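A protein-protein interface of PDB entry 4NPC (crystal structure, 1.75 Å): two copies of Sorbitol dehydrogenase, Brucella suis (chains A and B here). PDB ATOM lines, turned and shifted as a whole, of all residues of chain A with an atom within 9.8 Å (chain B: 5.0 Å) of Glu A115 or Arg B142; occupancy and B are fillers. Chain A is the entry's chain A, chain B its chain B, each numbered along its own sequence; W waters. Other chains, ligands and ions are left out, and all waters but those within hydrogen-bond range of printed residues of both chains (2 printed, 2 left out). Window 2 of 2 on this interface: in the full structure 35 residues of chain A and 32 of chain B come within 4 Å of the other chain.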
ATOM      1  N   LEU A 111     -14.161  20.568 -39.190  1.00  0.00           N
ATOM      2  CA  LEU A 111     -14.238  20.324 -37.753  1.00  0.00           C
ATOM      3  C   LEU A 111     -13.298  21.200 -36.951  1.00  0.00           C
ATOM      4  O   LEU A 111     -12.148  21.462 -37.377  1.00  0.00           O
ATOM      5  CB  LEU A 111     -13.898  18.857 -37.475  1.00  0.00           C
ATOM      6  CG  LEU A 111     -14.751  17.812 -38.206  1.00  0.00           C
ATOM      7  CD1 LEU A 111     -14.319  16.377 -37.919  1.00  0.00           C
ATOM      8  CD2 LEU A 111     -16.254  18.000 -37.930  1.00  0.00           C
ATOM      9  N   ALA A 112     -13.766  21.601 -35.769  1.00  0.00           N
ATOM     10  CA  ALA A 112     -12.956  22.344 -34.814  1.00  0.00           C
ATOM     11  C   ALA A 112     -13.719  22.443 -33.500  1.00  0.00           C
ATOM     12  O   ALA A 112     -14.964  22.377 -33.500  1.00  0.00           O
ATOM     13  CB  ALA A 112     -12.603  23.735 -35.329  1.00  0.00           C
ATOM     14  N   PRO A 113     -12.989  22.616 -32.387  1.00  0.00           N
ATOM     15  CA  PRO A 113     -13.716  22.828 -31.146  1.00  0.00           C
ATOM     16  C   PRO A 113     -14.688  24.006 -31.256  1.00  0.00           C
ATOM     17  O   PRO A 113     -14.426  24.992 -31.950  1.00  0.00           O
ATOM     18  CB  PRO A 113     -12.603  23.119 -30.106  1.00  0.00           C
ATOM     19  CG  PRO A 113     -11.376  22.532 -30.696  1.00  0.00           C
ATOM     20  CD  PRO A 113     -11.521  22.661 -32.182  1.00  0.00           C
ATOM     21  N   ALA A 114     -15.804  23.888 -30.558  1.00  0.00           N
ATOM     22  CA  ALA A 114     -16.890  24.840 -30.742  1.00  0.00           C
ATOM     23  C   ALA A 114     -16.476  26.296 -30.393  1.00  0.00           C
ATOM     24  O   ALA A 114     -16.887  27.226 -31.050  1.00  0.00           O
ATOM     25  CB  ALA A 114     -18.081  24.391 -29.947  1.00  0.00           C
ATOM     26  N   GLU A 115     -15.632  26.461 -29.395  1.00  0.00           N
ATOM     27  CA  GLU A 115     -15.180  27.802 -29.005  1.00  0.00           C
ATOM     28  C   GLU A 115     -14.165  28.400 -30.003  1.00  0.00           C
ATOM     29  O   GLU A 115     -13.870  29.593 -29.931  1.00  0.00           O
ATOM     30  CB  GLU A 115     -14.583  27.792 -27.593  1.00  0.00           C
ATOM     31  CG  GLU A 115     -13.371  26.891 -27.393  1.00  0.00           C
ATOM     32  CD  GLU A 115     -13.686  25.454 -26.946  1.00  0.00           C
ATOM     33  OE1 GLU A 115     -14.780  24.881 -27.188  1.00  0.00           O
ATOM     34  OE2 GLU A 115     -12.759  24.859 -26.320  1.00  0.00           O
ATOM     35  N   ASP A 116     -13.602  27.568 -30.877  1.00  0.00           N
ATOM     36  CA  ASP A 116     -12.557  27.992 -31.841  1.00  0.00           C
ATOM     37  C   ASP A 116     -13.030  28.110 -33.285  1.00  0.00           C
ATOM     38  O   ASP A 116     -12.408  28.838 -34.053  1.00  0.00           O
ATOM     39  CB  ASP A 116     -11.392  26.973 -31.831  1.00  0.00           C
ATOM     40  CG  ASP A 116     -10.674  26.892 -30.483  1.00  0.00           C
ATOM     41  OD1 ASP A 116     -10.642  27.895 -29.730  1.00  0.00           O
ATOM     42  OD2 ASP A 116     -10.182  25.783 -30.163  1.00  0.00           O
ATOM     43  N   ILE A 117     -14.092  27.384 -33.660  1.00  0.00           N
ATOM     44  CA  ILE A 117     -14.392  27.147 -35.072  1.00  0.00           C
ATOM     45  C   ILE A 117     -14.582  28.471 -35.834  1.00  0.00           C
ATOM     46  O   ILE A 117     -15.280  29.369 -35.349  1.00  0.00           O
ATOM     47  CB  ILE A 117     -15.573  26.152 -35.260  1.00  0.00           C
ATOM     48  CG1 ILE A 117     -15.668  25.743 -36.720  1.00  0.00           C
ATOM     49  CG2 ILE A 117     -16.888  26.731 -34.745  1.00  0.00           C
ATOM     50  CD1 ILE A 117     -16.531  24.517 -36.928  1.00  0.00           C
ATOM     51  N   SER A 118     -13.922  28.617 -36.982  1.00  0.00           N
ATOM     52  CA  SER A 118     -13.935  29.894 -37.697  1.00  0.00           C
ATOM     53  C   SER A 118     -15.255  30.136 -38.390  1.00  0.00           C
ATOM     54  O   SER A 118     -15.971  29.182 -38.761  1.00  0.00           O
ATOM     55  CB  SER A 118     -12.816  29.994 -38.746  1.00  0.00           C
ATOM     56  OG  SER A 118     -13.062  29.106 -39.805  1.00  0.00           O
ATOM     57  N   LEU A 119     -15.582  31.404 -38.602  1.00  0.00           N
ATOM     58  CA  LEU A 119     -16.764  31.724 -39.426  1.00  0.00           C
ATOM     59  C   LEU A 119     -16.652  31.157 -40.854  1.00  0.00           C
ATOM     60  O   LEU A 119     -17.639  30.819 -41.493  1.00  0.00           O
ATOM     61  CB  LEU A 119     -16.977  33.246 -39.481  1.00  0.00           C
ATOM     62  CG  LEU A 119     -18.284  33.729 -40.145  1.00  0.00           C
ATOM     63  CD1 LEU A 119     -19.539  33.085 -39.578  1.00  0.00           C
ATOM     64  CD2 LEU A 119     -18.430  35.246 -40.056  1.00  0.00           C
ATOM     65  N   ASP A 120     -15.433  31.090 -41.386  1.00  0.00           N
ATOM     66  CA  ASP A 120     -15.228  30.473 -42.689  1.00  0.00           C
ATOM     67  C   ASP A 120     -15.651  28.976 -42.695  1.00  0.00           C
ATOM     68  O   ASP A 120     -16.307  28.508 -43.638  1.00  0.00           O
ATOM     69  CB  ASP A 120     -13.756  30.629 -43.103  1.00  0.00           C
ATOM     70  CG  ASP A 120     -13.513  30.268 -44.562  1.00  0.00           C
ATOM     71  OD1 ASP A 120     -14.208  30.808 -45.445  1.00  0.00           O
ATOM     72  OD2 ASP A 120     -12.612  29.452 -44.817  1.00  0.00           O
ATOM     73  N   GLU A 166     -18.586  15.868 -30.756  1.00  0.00           N
ATOM     74  CA  GLU A 166     -17.558  16.877 -30.478  1.00  0.00           C
ATOM     75  C   GLU A 166     -16.808  17.309 -31.746  1.00  0.00           C
ATOM     76  O   GLU A 166     -16.455  16.449 -32.614  1.00  0.00           O
ATOM     77  CB  GLU A 166     -16.560  16.350 -29.413  1.00  0.00           C
ATOM     78  CG  GLU A 166     -17.268  15.912 -28.130  1.00  0.00           C
ATOM     79  CD  GLU A 166     -17.691  14.405 -28.086  1.00  0.00           C
ATOM     80  OE1 GLU A 166     -18.070  13.746 -29.147  1.00  0.00           O
ATOM     81  OE2 GLU A 166     -17.662  13.894 -26.913  1.00  0.00           O
ATOM     82  N   GLU A 167     -16.586  18.634 -31.835  1.00  0.00           N
ATOM     83  CA  GLU A 167     -15.957  19.349 -32.974  1.00  0.00           C
ATOM     84  C   GLU A 167     -16.871  19.522 -34.213  1.00  0.00           C
ATOM     85  O   GLU A 167     -16.464  20.099 -35.228  1.00  0.00           O
ATOM     86  CB  GLU A 167     -14.595  18.741 -33.412  1.00  0.00           C
ATOM     87  CG  GLU A 167     -13.580  18.660 -32.269  1.00  0.00           C
ATOM     88  CD  GLU A 167     -12.129  18.810 -32.713  1.00  0.00           C
ATOM     89  OE1 GLU A 167     -11.821  19.089 -33.879  1.00  0.00           O
ATOM     90  OE2 GLU A 167     -11.257  18.620 -31.866  1.00  0.00           O
ATOM     91  N   HIS A 168     -18.101  19.032 -34.112  1.00  0.00           N
ATOM     92  CA  HIS A 168     -19.020  19.060 -35.232  1.00  0.00           C
ATOM     93  C   HIS A 168     -20.100  20.131 -35.069  1.00  0.00           C
ATOM     94  O   HIS A 168     -21.234  19.942 -35.566  1.00  0.00           O
ATOM     95  CB  HIS A 168     -19.678  17.675 -35.403  1.00  0.00           C
ATOM     96  CG  HIS A 168     -18.785  16.571 -35.906  1.00  0.00           C
ATOM     97  ND1 HIS A 168     -17.702  16.072 -35.203  1.00  0.00           N
ATOM     98  CD2 HIS A 168     -18.866  15.823 -37.038  1.00  0.00           C
ATOM     99  CE1 HIS A 168     -17.149  15.088 -35.893  1.00  0.00           C
ATOM    100  NE2 HIS A 168     -17.839  14.914 -37.007  1.00  0.00           N
ATOM    101  N   VAL A 169     -19.839  21.271 -34.422  1.00  0.00           N
ATOM    102  CA  VAL A 169     -20.920  22.248 -34.227  1.00  0.00           C
ATOM    103  C   VAL A 169     -21.564  22.686 -35.570  1.00  0.00           C
ATOM    104  O   VAL A 169     -22.795  22.738 -35.738  1.00  0.00           O
ATOM    105  CB  VAL A 169     -20.504  23.407 -33.299  1.00  0.00           C
ATOM    106  CG1 VAL A 169     -19.450  24.300 -33.904  1.00  0.00           C
ATOM    107  CG2 VAL A 169     -21.728  24.225 -32.923  1.00  0.00           C
ATOM    108  N   ALA A 170     -20.738  22.977 -36.554  1.00  0.00           N
ATOM    109  CA  ALA A 170     -21.258  23.427 -37.848  1.00  0.00           C
ATOM    110  C   ALA A 170     -21.855  22.265 -38.604  1.00  0.00           C
ATOM    111  O   ALA A 170     -22.882  22.417 -39.264  1.00  0.00           O
ATOM    112  CB  ALA A 170     -20.143  24.074 -38.675  1.00  0.00           C
ATOM    113  N   ASN B  86     -19.291  40.495 -31.412  1.00  0.00           N
ATOM    114  CA  ASN B  86     -18.075  40.497 -30.560  1.00  0.00           C
ATOM    115  C   ASN B  86     -17.963  41.828 -29.788  1.00  0.00           C
ATOM    116  O   ASN B  86     -17.610  41.865 -28.573  1.00  0.00           O
ATOM    117  CB  ASN B  86     -16.807  40.210 -31.355  1.00  0.00           C
ATOM    118  CG  ASN B  86     -16.680  38.748 -31.772  1.00  0.00           C
ATOM    119  OD1 ASN B  86     -17.407  37.888 -31.300  1.00  0.00           O
ATOM    120  ND2 ASN B  86     -15.746  38.472 -32.661  1.00  0.00           N
ATOM    121  N   THR B 137     -23.746  32.561 -29.333  1.00  0.00           N
ATOM    122  CA  THR B 137     -23.419  31.484 -28.426  1.00  0.00           C
ATOM    123  C   THR B 137     -21.917  31.311 -28.339  1.00  0.00           C
ATOM    124  O   THR B 137     -21.376  31.130 -27.245  1.00  0.00           O
ATOM    125  CB  THR B 137     -24.065  30.140 -28.882  1.00  0.00           C
ATOM    126  OG1 THR B 137     -25.496  30.252 -28.899  1.00  0.00           O
ATOM    127  CG2 THR B 137     -23.673  29.018 -27.950  1.00  0.00           C
ATOM    128  N   GLN B 138     -21.225  31.412 -29.462  1.00  0.00           N
ATOM    129  CA  GLN B 138     -19.775  31.280 -29.438  1.00  0.00           C
ATOM    130  C   GLN B 138     -19.098  32.422 -28.635  1.00  0.00           C
ATOM    131  O   GLN B 138     -18.213  32.172 -27.815  1.00  0.00           O
ATOM    132  CB  GLN B 138     -19.180  31.213 -30.844  1.00  0.00           C
ATOM    133  CG  GLN B 138     -17.748  30.735 -30.856  1.00  0.00           C
ATOM    134  CD  GLN B 138     -17.153  30.730 -32.252  1.00  0.00           C
ATOM    135  OE1 GLN B 138     -17.274  31.713 -32.984  1.00  0.00           O
ATOM    136  NE2 GLN B 138     -16.588  29.595 -32.663  1.00  0.00           N
ATOM    137  N   ALA B 139     -19.501  33.664 -28.892  1.00  0.00           N
ATOM    138  CA  ALA B 139     -18.883  34.816 -28.199  1.00  0.00           C
ATOM    139  C   ALA B 139     -19.150  34.789 -26.697  1.00  0.00           C
ATOM    140  O   ALA B 139     -18.223  34.982 -25.896  1.00  0.00           O
ATOM    141  CB  ALA B 139     -19.361  36.128 -28.782  1.00  0.00           C
ATOM    142  N   VAL B 140     -20.394  34.513 -26.328  1.00  0.00           N
ATOM    143  CA  VAL B 140     -20.755  34.412 -24.913  1.00  0.00           C
ATOM    144  C   VAL B 140     -20.025  33.262 -24.233  1.00  0.00           C
ATOM    145  O   VAL B 140     -19.479  33.426 -23.136  1.00  0.00           O
ATOM    146  CB  VAL B 140     -22.265  34.220 -24.720  1.00  0.00           C
ATOM    147  CG1 VAL B 140     -22.559  33.935 -23.261  1.00  0.00           C
ATOM    148  CG2 VAL B 140     -23.007  35.448 -25.184  1.00  0.00           C
ATOM    149  N   GLY B 141     -20.004  32.102 -24.893  1.00  0.00           N
ATOM    150  CA  GLY B 141     -19.360  30.916 -24.319  1.00  0.00           C
ATOM    151  C   GLY B 141     -17.888  31.112 -24.103  1.00  0.00           C
ATOM    152  O   GLY B 141     -17.319  30.687 -23.067  1.00  0.00           O
ATOM    153  N   ARG B 142     -17.229  31.773 -25.052  1.00  0.00           N
ATOM    154  CA  ARG B 142     -15.825  32.118 -24.832  1.00  0.00           C
ATOM    155  C   ARG B 142     -15.640  32.909 -23.530  1.00  0.00           C
ATOM    156  O   ARG B 142     -14.712  32.680 -22.786  1.00  0.00           O
ATOM    157  CB  ARG B 142     -15.293  32.938 -26.011  1.00  0.00           C
ATOM    158  CG  ARG B 142     -15.064  32.104 -27.252  1.00  0.00           C
ATOM    159  CD  ARG B 142     -14.774  33.004 -28.454  1.00  0.00           C
ATOM    160  NE  ARG B 142     -14.373  32.226 -29.616  1.00  0.00           N
ATOM    161  CZ  ARG B 142     -14.371  32.664 -30.875  1.00  0.00           C
ATOM    162  NH1 ARG B 142     -14.760  33.904 -31.156  1.00  0.00           N
ATOM    163  NH2 ARG B 142     -13.987  31.852 -31.863  1.00  0.00           N
ATOM    164  N   ALA B 143     -16.479  33.904 -23.308  1.00  0.00           N
ATOM    165  CA  ALA B 143     -16.329  34.722 -22.135  1.00  0.00           C
ATOM    166  C   ALA B 143     -16.572  33.866 -20.892  1.00  0.00           C
ATOM    167  O   ALA B 143     -15.897  34.023 -19.861  1.00  0.00           O
ATOM    168  CB  ALA B 143     -17.277  35.881 -22.181  1.00  0.00           C
ATOM    169  N   MET B 144     -17.570  32.986 -20.964  1.00  0.00           N
ATOM    170  CA  MET B 144     -17.910  32.138 -19.818  1.00  0.00           C
ATOM    171  C   MET B 144     -16.816  31.136 -19.481  1.00  0.00           C
ATOM    172  O   MET B 144     -16.519  30.889 -18.324  1.00  0.00           O
ATOM    173  CB  MET B 144     -19.191  31.360 -20.071  1.00  0.00           C
ATOM    174  CG  MET B 144     -20.414  32.234 -20.071  1.00  0.00           C
ATOM    175  SD  MET B 144     -21.888  31.336 -20.600  1.00  0.00           S
ATOM    176  CE  MET B 144     -23.172  32.579 -20.344  1.00  0.00           C
ATOM    177  N   ILE B 145     -16.213  30.565 -20.505  1.00  0.00           N
ATOM    178  CA  ILE B 145     -15.156  29.618 -20.308  1.00  0.00           C
ATOM    179  C   ILE B 145     -14.008  30.365 -19.618  1.00  0.00           C
ATOM    180  O   ILE B 145     -13.478  29.886 -18.602  1.00  0.00           O
ATOM    181  CB  ILE B 145     -14.708  29.018 -21.635  1.00  0.00           C
ATOM    182  CG1 ILE B 145     -15.780  28.079 -22.202  1.00  0.00           C
ATOM    183  CG2 ILE B 145     -13.389  28.283 -21.475  1.00  0.00           C
ATOM    184  CD1 ILE B 145     -15.570  27.777 -23.681  1.00  0.00           C
ATOM    185  N   ALA B 146     -13.661  31.543 -20.138  1.00  0.00           N
ATOM    186  CA  ALA B 146     -12.540  32.300 -19.597  1.00  0.00           C
ATOM    187  C   ALA B 146     -12.751  32.674 -18.142  1.00  0.00           C
ATOM    188  O   ALA B 146     -11.809  32.680 -17.354  1.00  0.00           O
ATOM    189  CB  ALA B 146     -12.262  33.546 -20.438  1.00  0.00           C
ATOM    190  N   GLU B 188     -19.944  19.839 -25.717  1.00  0.00           N
ATOM    191  CA  GLU B 188     -18.545  20.278 -25.565  1.00  0.00           C
ATOM    192  C   GLU B 188     -18.292  21.113 -24.345  1.00  0.00           C
ATOM    193  O   GLU B 188     -17.134  21.175 -23.857  1.00  0.00           O
ATOM    194  CB  GLU B 188     -18.091  21.088 -26.767  1.00  0.00           C
ATOM    195  CG  GLU B 188     -18.084  20.280 -28.055  1.00  0.00           C
ATOM    196  CD  GLU B 188     -17.370  20.935 -29.204  1.00  0.00           C
ATOM    197  OE1 GLU B 188     -16.375  21.681 -28.970  1.00  0.00           O
ATOM    198  OE2 GLU B 188     -17.744  20.622 -30.357  1.00  0.00           O
ATOM    199  N   TRP B 189     -19.304  21.844 -23.905  1.00  0.00           N
ATOM    200  CA  TRP B 189     -19.097  22.826 -22.809  1.00  0.00           C
ATOM    201  C   TRP B 189     -19.617  22.416 -21.407  1.00  0.00           C
ATOM    202  O   TRP B 189     -19.417  23.151 -20.437  1.00  0.00           O
ATOM    203  CB  TRP B 189     -19.660  24.163 -23.229  1.00  0.00           C
ATOM    204  CG  TRP B 189     -18.925  24.806 -24.346  1.00  0.00           C
ATOM    205  CD1 TRP B 189     -17.734  24.428 -24.893  1.00  0.00           C
ATOM    206  CD2 TRP B 189     -19.341  25.963 -25.058  1.00  0.00           C
ATOM    207  NE1 TRP B 189     -17.389  25.277 -25.904  1.00  0.00           N
ATOM    208  CE2 TRP B 189     -18.343  26.258 -25.991  1.00  0.00           C
ATOM    209  CE3 TRP B 189     -20.431  26.813 -24.948  1.00  0.00           C
ATOM    210  CZ2 TRP B 189     -18.443  27.324 -26.854  1.00  0.00           C
ATOM    211  CZ3 TRP B 189     -20.528  27.881 -25.798  1.00  0.00           C
ATOM    212  CH2 TRP B 189     -19.544  28.144 -26.719  1.00  0.00           C
ATOM    213  N   TYR B 192     -17.025  22.786 -18.841  1.00  0.00           N
ATOM    214  CA  TYR B 192     -16.832  24.148 -18.323  1.00  0.00           C
ATOM    215  C   TYR B 192     -18.030  24.688 -17.533  1.00  0.00           C
ATOM    216  O   TYR B 192     -18.068  25.874 -17.171  1.00  0.00           O
ATOM    217  CB  TYR B 192     -16.557  25.102 -19.466  1.00  0.00           C
ATOM    218  CG  TYR B 192     -15.413  24.646 -20.321  1.00  0.00           C
ATOM    219  CD1 TYR B 192     -14.195  24.346 -19.739  1.00  0.00           C
ATOM    220  CD2 TYR B 192     -15.552  24.466 -21.675  1.00  0.00           C
ATOM    221  CE1 TYR B 192     -13.141  23.893 -20.497  1.00  0.00           C
ATOM    222  CE2 TYR B 192     -14.492  24.019 -22.435  1.00  0.00           C
ATOM    223  CZ  TYR B 192     -13.287  23.750 -21.836  1.00  0.00           C
ATOM    224  OH  TYR B 192     -12.222  23.294 -22.583  1.00  0.00           O
HETATM  225  O   HOH W   1     -14.649  22.172 -26.988  1.00  0.00           O
HETATM  226  O   HOH W   2     -16.279  32.091 -35.493  1.00  0.00           O
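The backbone NH of Glu A167 sits at hydrogen-bond distance from the side-chain carboxylate of Glu B188 (2.7 Å).
The side-chain carboxylate (OE1) of Glu B188 lies within hydrogen-bond range of the backbone NH (N) of Ala A114.
The indole nitrogen (NE1) of Trp B189 lies within hydrogen-bond range of the side-chain carboxylate (OE1) of Glu A115, at 2.9 Å.
O of Glu A115 sits at hydrogen-bond distance from NE of Arg B142 (2.7 Å).
The side-chain amide nitrogen (NE2) of Gln B138 sits at hydrogen-bond distance from the backbone carbonyl oxygen (O) of Ala A114.
O of Ile A117 lies within hydrogen-bond range of NE2 of Gln B138 (3.0 Å).
O of Glu A167 sits at hydrogen-bond distance from N of Ala A112 (3.1 Å).
O of Glu A166 sits at hydrogen-bond distance from ND1 of His A168, 2.9 Å away.
The guanidinium group (NH2) of Arg B142 lies close to the side-chain amide oxygen (OE1) of Gln B138 (3.5 Å).
Among the printed residues, merely in contact across the chains: Pro A113 with Glu B188, Glu A166 with Glu B188, Glu A115 with Gln B138, Asp A116 with Gln B138 and Glu A115 with Glu B188.
Printed residues of chain B within 4 Å of Ala A114: Gln B138 and Glu B188.
Printed residues of chain B within 4 Å of Glu A115: Gln B138 (3.8 Å), Arg B142 (2.7 Å), Glu B188 (3.99 Å) and Trp B189 (2.9 Å).
Printed residues of chain B within 4 Å of Ile A117: Gln B138 (3.0 Å).
Printed residues of chain B within 4 Å of Glu A166: Glu B188.
No residue of chain A comes within 4 Å of Ala B139.
Printed residues of chain A within 4 Å of Arg B142: Glu A115.
No residue of chain A comes within 4 Å of Ala B143.
Of the printed residues of chain A, Glu B188 touches Pro A113, Ala A114, Glu A115, Glu A166 and Glu A167.
The nearest printed residue of chain B that does not touch Glu A115 is Ile B145 (4.03 Å).
Hydrophobic or aromatic side chains of chain A that line the printed part of chain B: Ala A114 and Ile A117.
Hydrophobic or aromatic side chains of chain B within 4 Å of the printed part of chain A: Trp B189.
Among the printed residues, 11 pairs touch across the chains.
No position is printed for both chains.
Of the 11 pairs that touch across the chains among the printed residues, none has its exchanged pair printed and touching as well.
Water W1 lies within hydrogen-bond range of the side-chain carboxylate (OE1) of Glu B188 (2.7 Å) and the side-chain carboxylate (OE1) of Glu A115 (2.7 Å).
Water W2 lies within hydrogen-bond range of OE1 of Gln B138 (2.7 Å), O of Ile A117 (2.9 Å) and N of Leu A119 (3.3 Å).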
